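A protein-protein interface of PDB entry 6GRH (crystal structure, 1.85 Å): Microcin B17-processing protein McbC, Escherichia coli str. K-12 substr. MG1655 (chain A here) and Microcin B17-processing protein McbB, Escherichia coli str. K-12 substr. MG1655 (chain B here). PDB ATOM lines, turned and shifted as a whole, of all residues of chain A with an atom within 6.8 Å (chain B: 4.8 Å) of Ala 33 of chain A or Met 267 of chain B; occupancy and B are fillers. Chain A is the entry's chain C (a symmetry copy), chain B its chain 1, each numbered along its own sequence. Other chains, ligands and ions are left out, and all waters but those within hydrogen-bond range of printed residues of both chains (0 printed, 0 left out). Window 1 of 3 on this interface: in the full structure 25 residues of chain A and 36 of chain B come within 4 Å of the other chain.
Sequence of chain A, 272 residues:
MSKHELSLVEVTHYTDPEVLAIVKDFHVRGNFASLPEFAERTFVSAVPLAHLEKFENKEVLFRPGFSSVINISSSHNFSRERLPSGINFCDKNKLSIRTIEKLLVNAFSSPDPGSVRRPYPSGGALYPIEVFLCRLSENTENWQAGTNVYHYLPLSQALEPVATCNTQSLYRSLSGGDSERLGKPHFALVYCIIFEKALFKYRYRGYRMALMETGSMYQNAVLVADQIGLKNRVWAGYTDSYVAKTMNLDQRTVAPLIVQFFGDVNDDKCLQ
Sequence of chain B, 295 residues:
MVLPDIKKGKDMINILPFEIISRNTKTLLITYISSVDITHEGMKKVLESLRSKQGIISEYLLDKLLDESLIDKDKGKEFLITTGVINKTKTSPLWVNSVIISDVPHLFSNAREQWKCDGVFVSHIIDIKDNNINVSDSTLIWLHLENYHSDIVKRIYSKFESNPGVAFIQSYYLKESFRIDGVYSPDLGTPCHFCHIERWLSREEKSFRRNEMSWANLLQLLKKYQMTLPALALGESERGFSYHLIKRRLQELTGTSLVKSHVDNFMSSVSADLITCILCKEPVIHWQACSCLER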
ATOM      1  N   ASN A  31       7.184  15.236 -22.890  1.00  0.00           N
ATOM      2  CA  ASN A  31       7.462  13.817 -23.012  1.00  0.00           C
ATOM      3  C   ASN A  31       8.423  13.434 -21.877  1.00  0.00           C
ATOM      4  O   ASN A  31       9.260  14.233 -21.486  1.00  0.00           O
ATOM      5  CB  ASN A  31       8.099  13.499 -24.362  1.00  0.00           C
ATOM      6  CG  ASN A  31       7.096  13.464 -25.529  1.00  0.00           C
ATOM      7  OD1 ASN A  31       5.885  13.513 -25.369  1.00  0.00           O
ATOM      8  ND2 ASN A  31       7.622  13.342 -26.696  1.00  0.00           N
ATOM      9  N   PHE A  32       8.358  12.176 -21.455  1.00  0.00           N
ATOM     10  CA  PHE A  32       9.133  11.646 -20.340  1.00  0.00           C
ATOM     11  C   PHE A  32      10.060  10.555 -20.830  1.00  0.00           C
ATOM     12  O   PHE A  32       9.764   9.889 -21.805  1.00  0.00           O
ATOM     13  CB  PHE A  32       8.185  11.015 -19.298  1.00  0.00           C
ATOM     14  CG  PHE A  32       7.593  11.969 -18.295  1.00  0.00           C
ATOM     15  CD1 PHE A  32       7.759  13.355 -18.370  1.00  0.00           C
ATOM     16  CD2 PHE A  32       6.825  11.451 -17.247  1.00  0.00           C
ATOM     17  CE1 PHE A  32       7.183  14.190 -17.434  1.00  0.00           C
ATOM     18  CE2 PHE A  32       6.249  12.286 -16.295  1.00  0.00           C
ATOM     19  CZ  PHE A  32       6.436  13.662 -16.384  1.00  0.00           C
ATOM     20  N   ALA A  33      11.204  10.444 -20.183  1.00  0.00           N
ATOM     21  CA  ALA A  33      12.050   9.258 -20.207  1.00  0.00           C
ATOM     22  C   ALA A  33      11.887   8.602 -18.845  1.00  0.00           C
ATOM     23  O   ALA A  33      12.551   8.954 -17.888  1.00  0.00           O
ATOM     24  CB  ALA A  33      13.492   9.643 -20.459  1.00  0.00           C
ATOM     25  N   SER A  34      10.969   7.650 -18.772  1.00  0.00           N
ATOM     26  CA  SER A  34      10.574   7.026 -17.531  1.00  0.00           C
ATOM     27  C   SER A  34      10.854   5.537 -17.668  1.00  0.00           C
ATOM     28  O   SER A  34      10.081   4.809 -18.270  1.00  0.00           O
ATOM     29  CB  SER A  34       9.087   7.278 -17.321  1.00  0.00           C
ATOM     30  OG  SER A  34       8.625   6.542 -16.207  1.00  0.00           O
ATOM     31  N   LEU A  35      11.969   5.085 -17.144  1.00  0.00           N
ATOM     32  CA  LEU A  35      12.351   3.667 -17.256  1.00  0.00           C
ATOM     33  C   LEU A  35      12.874   3.177 -15.928  1.00  0.00           C
ATOM     34  O   LEU A  35      13.465   3.955 -15.208  1.00  0.00           O
ATOM     35  CB  LEU A  35      13.481   3.509 -18.270  1.00  0.00           C
ATOM     36  CG  LEU A  35      13.236   3.819 -19.741  1.00  0.00           C
ATOM     37  CD1 LEU A  35      14.525   3.549 -20.493  1.00  0.00           C
ATOM     38  CD2 LEU A  35      12.138   2.924 -20.298  1.00  0.00           C
ATOM     39  N   PHE A  38      16.528   4.094 -15.096  1.00  0.00           N
ATOM     40  CA  PHE A  38      16.861   5.471 -14.729  1.00  0.00           C
ATOM     41  C   PHE A  38      16.342   5.903 -13.334  1.00  0.00           C
ATOM     42  O   PHE A  38      16.346   7.102 -13.036  1.00  0.00           O
ATOM     43  CB  PHE A  38      16.300   6.453 -15.766  1.00  0.00           C
ATOM     44  CG  PHE A  38      16.727   6.202 -17.199  1.00  0.00           C
ATOM     45  CD1 PHE A  38      17.922   5.577 -17.530  1.00  0.00           C
ATOM     46  CD2 PHE A  38      15.921   6.679 -18.231  1.00  0.00           C
ATOM     47  CE1 PHE A  38      18.279   5.379 -18.854  1.00  0.00           C
ATOM     48  CE2 PHE A  38      16.278   6.497 -19.564  1.00  0.00           C
ATOM     49  CZ  PHE A  38      17.465   5.838 -19.871  1.00  0.00           C
ATOM     50  N   THR A  42      16.909  10.082 -12.005  1.00  0.00           N
ATOM     51  CA  THR A  42      15.844  10.990 -12.463  1.00  0.00           C
ATOM     52  C   THR A  42      14.792  11.167 -11.384  1.00  0.00           C
ATOM     53  O   THR A  42      14.730  10.394 -10.429  1.00  0.00           O
ATOM     54  CB  THR A  42      15.149  10.446 -13.737  1.00  0.00           C
ATOM     55  OG1 THR A  42      14.622   9.130 -13.497  1.00  0.00           O
ATOM     56  CG2 THR A  42      16.127  10.393 -14.896  1.00  0.00           C
ATOM     57  N   TYR A 238       4.990   7.043 -18.412  1.00  0.00           N
ATOM     58  CA  TYR A 238       5.559   6.205 -19.466  1.00  0.00           C
ATOM     59  C   TYR A 238       6.483   7.051 -20.324  1.00  0.00           C
ATOM     60  O   TYR A 238       6.410   8.302 -20.320  1.00  0.00           O
ATOM     61  CB  TYR A 238       4.448   5.543 -20.308  1.00  0.00           C
ATOM     62  CG  TYR A 238       3.583   6.522 -21.037  1.00  0.00           C
ATOM     63  CD1 TYR A 238       3.936   6.986 -22.300  1.00  0.00           C
ATOM     64  CD2 TYR A 238       2.449   7.050 -20.437  1.00  0.00           C
ATOM     65  CE1 TYR A 238       3.164   7.927 -22.956  1.00  0.00           C
ATOM     66  CE2 TYR A 238       1.670   7.959 -21.078  1.00  0.00           C
ATOM     67  CZ  TYR A 238       2.034   8.403 -22.342  1.00  0.00           C
ATOM     68  OH  TYR A 238       1.259   9.345 -22.989  1.00  0.00           O
ATOM     69  N   THR A 239       7.303   6.359 -21.102  1.00  0.00           N
ATOM     70  CA  THR A 239       8.225   6.976 -22.029  1.00  0.00           C
ATOM     71  C   THR A 239       7.533   7.061 -23.382  1.00  0.00           C
ATOM     72  O   THR A 239       7.337   6.044 -24.046  1.00  0.00           O
ATOM     73  CB  THR A 239       9.514   6.143 -22.135  1.00  0.00           C
ATOM     74  OG1 THR A 239      10.098   6.038 -20.827  1.00  0.00           O
ATOM     75  CG2 THR A 239      10.499   6.801 -23.113  1.00  0.00           C
ATOM     76  N   ASP A 240       7.138   8.265 -23.765  1.00  0.00           N
ATOM     77  CA  ASP A 240       6.274   8.465 -24.932  1.00  0.00           C
ATOM     78  C   ASP A 240       6.854   7.868 -26.224  1.00  0.00           C
ATOM     79  O   ASP A 240       6.150   7.199 -26.965  1.00  0.00           O
ATOM     80  CB  ASP A 240       5.936   9.947 -25.155  1.00  0.00           C
ATOM     81  CG  ASP A 240       5.401  10.641 -23.891  1.00  0.00           C
ATOM     82  OD1 ASP A 240       6.127  10.694 -22.861  1.00  0.00           O
ATOM     83  OD2 ASP A 240       4.247  11.141 -23.938  1.00  0.00           O
ATOM     84  N   SER A 241       8.130   8.104 -26.482  1.00  0.00           N
ATOM     85  CA  SER A 241       8.727   7.689 -27.735  1.00  0.00           C
ATOM     86  C   SER A 241       8.867   6.165 -27.794  1.00  0.00           C
ATOM     87  O   SER A 241       8.758   5.559 -28.862  1.00  0.00           O
ATOM     88  CB  SER A 241      10.077   8.362 -27.927  1.00  0.00           C
ATOM     89  OG  SER A 241      10.945   7.982 -26.895  1.00  0.00           O
ATOM     90  N   GLY B 182      20.817  14.976 -28.092  1.00  0.00           N
ATOM     91  CA  GLY B 182      20.093  14.044 -27.254  1.00  0.00           C
ATOM     92  C   GLY B 182      20.516  12.618 -27.555  1.00  0.00           C
ATOM     93  O   GLY B 182      21.086  12.327 -28.603  1.00  0.00           O
ATOM     94  N   VAL B 183      20.174  11.718 -26.659  1.00  0.00           N
ATOM     95  CA  VAL B 183      20.540  10.338 -26.832  1.00  0.00           C
ATOM     96  C   VAL B 183      19.675   9.773 -27.939  1.00  0.00           C
ATOM     97  O   VAL B 183      18.452   9.857 -27.870  1.00  0.00           O
ATOM     98  CB  VAL B 183      20.312   9.525 -25.554  1.00  0.00           C
ATOM     99  CG1 VAL B 183      20.638   8.057 -25.826  1.00  0.00           C
ATOM    100  CG2 VAL B 183      21.173  10.045 -24.418  1.00  0.00           C
ATOM    101  N   SER B 185      18.493   6.452 -29.349  1.00  0.00           N
ATOM    102  CA  SER B 185      18.281   5.052 -29.010  1.00  0.00           C
ATOM    103  C   SER B 185      17.226   4.501 -29.948  1.00  0.00           C
ATOM    104  O   SER B 185      16.050   4.876 -29.836  1.00  0.00           O
ATOM    105  CB  SER B 185      17.805   4.912 -27.578  1.00  0.00           C
ATOM    106  OG  SER B 185      17.295   3.604 -27.323  1.00  0.00           O
ATOM    107  N   LEU B 188      14.364   2.951 -27.995  1.00  0.00           N
ATOM    108  CA  LEU B 188      13.447   3.943 -27.375  1.00  0.00           C
ATOM    109  C   LEU B 188      12.738   4.920 -28.333  1.00  0.00           C
ATOM    110  O   LEU B 188      11.874   5.694 -27.896  1.00  0.00           O
ATOM    111  CB  LEU B 188      14.188   4.719 -26.293  1.00  0.00           C
ATOM    112  CG  LEU B 188      14.692   3.894 -25.108  1.00  0.00           C
ATOM    113  CD1 LEU B 188      15.563   4.757 -24.218  1.00  0.00           C
ATOM    114  CD2 LEU B 188      13.577   3.270 -24.269  1.00  0.00           C
ATOM    115  N   THR B 190      13.960   7.573 -30.078  1.00  0.00           N
ATOM    116  CA  THR B 190      14.321   8.985 -29.917  1.00  0.00           C
ATOM    117  C   THR B 190      15.034   9.533 -31.172  1.00  0.00           C
ATOM    118  O   THR B 190      15.598   8.750 -31.947  1.00  0.00           O
ATOM    119  CB  THR B 190      15.244   9.215 -28.706  1.00  0.00           C
ATOM    120  OG1 THR B 190      16.404   8.404 -28.817  1.00  0.00           O
ATOM    121  CG2 THR B 190      14.538   8.884 -27.403  1.00  0.00           C
ATOM    122  N   ARG B 249      27.983  14.846 -18.835  1.00  0.00           N
ATOM    123  CA  ARG B 249      26.887  14.217 -19.522  1.00  0.00           C
ATOM    124  C   ARG B 249      26.929  12.690 -19.412  1.00  0.00           C
ATOM    125  O   ARG B 249      25.914  12.050 -19.135  1.00  0.00           O
ATOM    126  CB  ARG B 249      26.803  14.740 -20.976  1.00  0.00           C
ATOM    127  CG  ARG B 249      25.588  14.236 -21.713  1.00  0.00           C
ATOM    128  CD  ARG B 249      24.334  14.914 -21.199  1.00  0.00           C
ATOM    129  NE  ARG B 249      23.169  14.407 -21.899  1.00  0.00           N
ATOM    130  CZ  ARG B 249      22.066  13.908 -21.351  1.00  0.00           C
ATOM    131  NH1 ARG B 249      21.875  13.871 -20.023  1.00  0.00           N
ATOM    132  NH2 ARG B 249      21.104  13.468 -22.162  1.00  0.00           N
ATOM    133  N   VAL B 263      12.579  13.783 -15.489  1.00  0.00           N
ATOM    134  CA  VAL B 263      12.327  12.831 -16.561  1.00  0.00           C
ATOM    135  C   VAL B 263      12.001  13.513 -17.918  1.00  0.00           C
ATOM    136  O   VAL B 263      12.248  12.945 -18.957  1.00  0.00           O
ATOM    137  CB  VAL B 263      11.201  11.821 -16.195  1.00  0.00           C
ATOM    138  CG1 VAL B 263      11.708  10.817 -15.166  1.00  0.00           C
ATOM    139  CG2 VAL B 263       9.939  12.495 -15.703  1.00  0.00           C
ATOM    140  N   ASN B 265      13.570  15.948 -19.381  1.00  0.00           N
ATOM    141  CA  ASN B 265      14.743  16.477 -20.075  1.00  0.00           C
ATOM    142  C   ASN B 265      16.016  15.652 -19.914  1.00  0.00           C
ATOM    143  O   ASN B 265      17.086  16.123 -20.290  1.00  0.00           O
ATOM    144  CB  ASN B 265      14.997  17.921 -19.611  1.00  0.00           C
ATOM    145  CG  ASN B 265      15.278  18.013 -18.117  1.00  0.00           C
ATOM    146  OD1 ASN B 265      14.598  18.745 -17.381  1.00  0.00           O
ATOM    147  ND2 ASN B 265      16.255  17.252 -17.661  1.00  0.00           N
ATOM    148  N   PHE B 266      15.905  14.437 -19.367  1.00  0.00           N
ATOM    149  CA  PHE B 266      17.072  13.567 -19.114  1.00  0.00           C
ATOM    150  C   PHE B 266      17.788  13.115 -20.401  1.00  0.00           C
ATOM    151  O   PHE B 266      19.010  13.063 -20.453  1.00  0.00           O
ATOM    152  CB  PHE B 266      16.593  12.343 -18.326  1.00  0.00           C
ATOM    153  CG  PHE B 266      17.670  11.361 -17.983  1.00  0.00           C
ATOM    154  CD1 PHE B 266      18.754  11.742 -17.215  1.00  0.00           C
ATOM    155  CD2 PHE B 266      17.586  10.046 -18.422  1.00  0.00           C
ATOM    156  CE1 PHE B 266      19.738  10.827 -16.872  1.00  0.00           C
ATOM    157  CE2 PHE B 266      18.580   9.120 -18.080  1.00  0.00           C
ATOM    158  CZ  PHE B 266      19.657   9.525 -17.316  1.00  0.00           C
ATOM    159  N   MET B 267      17.046  12.811 -21.447  1.00  0.00           N
ATOM    160  CA  MET B 267      17.698  12.390 -22.687  1.00  0.00           C
ATOM    161  C   MET B 267      17.849  13.488 -23.728  1.00  0.00           C
ATOM    162  O   MET B 267      18.212  13.197 -24.873  1.00  0.00           O
ATOM    163  CB  MET B 267      16.968  11.198 -23.259  1.00  0.00           C
ATOM    164  CG  MET B 267      17.160   9.978 -22.379  1.00  0.00           C
ATOM    165  SD  MET B 267      16.255   8.580 -23.037  1.00  0.00           S
ATOM    166  CE  MET B 267      16.918   8.439 -24.692  1.00  0.00           C
ATOM    167  N   SER B 268      17.577  14.740 -23.344  1.00  0.00           N
ATOM    168  CA  SER B 268      17.580  15.836 -24.306  1.00  0.00           C
ATOM    169  C   SER B 268      18.966  16.379 -24.682  1.00  0.00           C
ATOM    170  O   SER B 268      19.967  16.142 -24.000  1.00  0.00           O
ATOM    171  CB  SER B 268      16.723  16.990 -23.760  1.00  0.00           C
ATOM    172  OG  SER B 268      15.423  16.519 -23.554  1.00  0.00           O
ATOM    173  N   SER B 269      18.989  17.163 -25.759  1.00  0.00           N
ATOM    174  CA  SER B 269      20.201  17.801 -26.236  1.00  0.00           C
ATOM    175  C   SER B 269      20.688  18.852 -25.223  1.00  0.00           C
ATOM    176  O   SER B 269      19.896  19.414 -24.488  1.00  0.00           O
ATOM    177  CB  SER B 269      19.960  18.466 -27.596  1.00  0.00           C
ATOM    178  OG  SER B 269      19.172  19.639 -27.431  1.00  0.00           O
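The side-chain hydroxyl (OG) of Ser 185 of chain B sits at hydrogen-bond distance from the backbone NH (N) of Leu 188 of chain B (3.1 Å). O of Phe 38 of chain A is in hydrogen-bond range of OG1 of Thr 42 of chain A. The backbone carbonyl oxygen (O) of Val 183 of chain B is in hydrogen-bond range of the side-chain hydroxyl (OG1) of Thr 190 of chain B, 2.7 Å away. N of Val 183 of chain B is in hydrogen-bond range of O of Met 267 of chain B (3.0 Å). The backbone carbonyl oxygen (O) of Phe 266 of chain B is in hydrogen-bond range of the guanidinium group (NH2) of Arg 249 of chain B, at 2.7 Å. The side-chain hydroxyl of Thr 190 of chain B sits at hydrogen-bond distance from the backbone NH of Ser 185 of chain B (2.9 Å).
OG of Ser 241 of chain A is in hydrogen-bond range of O of Leu 188 of chain B, at 2.7 Å. N of Ala 33 of chain A lies within hydrogen-bond range of O of Val 263 of chain B, 3.0 Å away.
Hydrophobic or aromatic side chains of chain A that line the printed part of chain B: Phe 32, Ala 33, Leu 35 and Phe 38. Of the 12 printed residues of chain B, 5 touch a printed residue of chain A. Among the printed residues, no Asp or Glu carboxylate lies within 4 Å of a Lys or Arg side-chain nitrogen of the other chain.
Printed residues of chain B within 4 Å of Ala 33 of chain A: Val 263 (3.0 Å) and Met 267 (3.9 Å). Of the printed residues of chain B, Leu 35 of chain A touches Leu 188. Of the printed residues of chain B, Ser 241 of chain A touches Leu 188 and Thr 190. Of the printed residues of chain B, Thr 42 of chain A touches Val 263 (3.7 Å) and Phe 266 (3.6 Å). Of the printed residues of chain A, Val 263 of chain B touches Phe 32 (3.5 Å), Ala 33 (3.0 Å) and Thr 42 (3.7 Å). Of the printed residues of chain A, Phe 266 of chain B touches Phe 38 and Thr 42. Ser 34 of chain A touches none of the printed residues of chain B. The nearest printed residue of chain B that does not touch Ala 33 of chain A is Phe 266 of chain B (4.6 Å). The nearest printed residue of chain A that does not touch Met 267 of chain B is Phe 38 of chain A (4.05 Å).
Val 263 of chain B touches Phe 32 of chain A. Ala 33 of chain A touches Met 267 of chain B (CB to SD, 3.9 Å). Leu 188 of chain B touches Leu 35 of chain A (CD2 to CD1, 3.9 Å). CG of Phe 38 of chain A touches CE2 of Phe 266 of chain B, 3.6 Å away. Thr 42 of chain A touches Val 263 of chain B (CB to CG1, 3.7 Å). CG of Phe 266 of chain B touches CG2 of Thr 42 of chain A, at 3.6 Å. Thr 190 of chain B touches Ser 241 of chain A.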
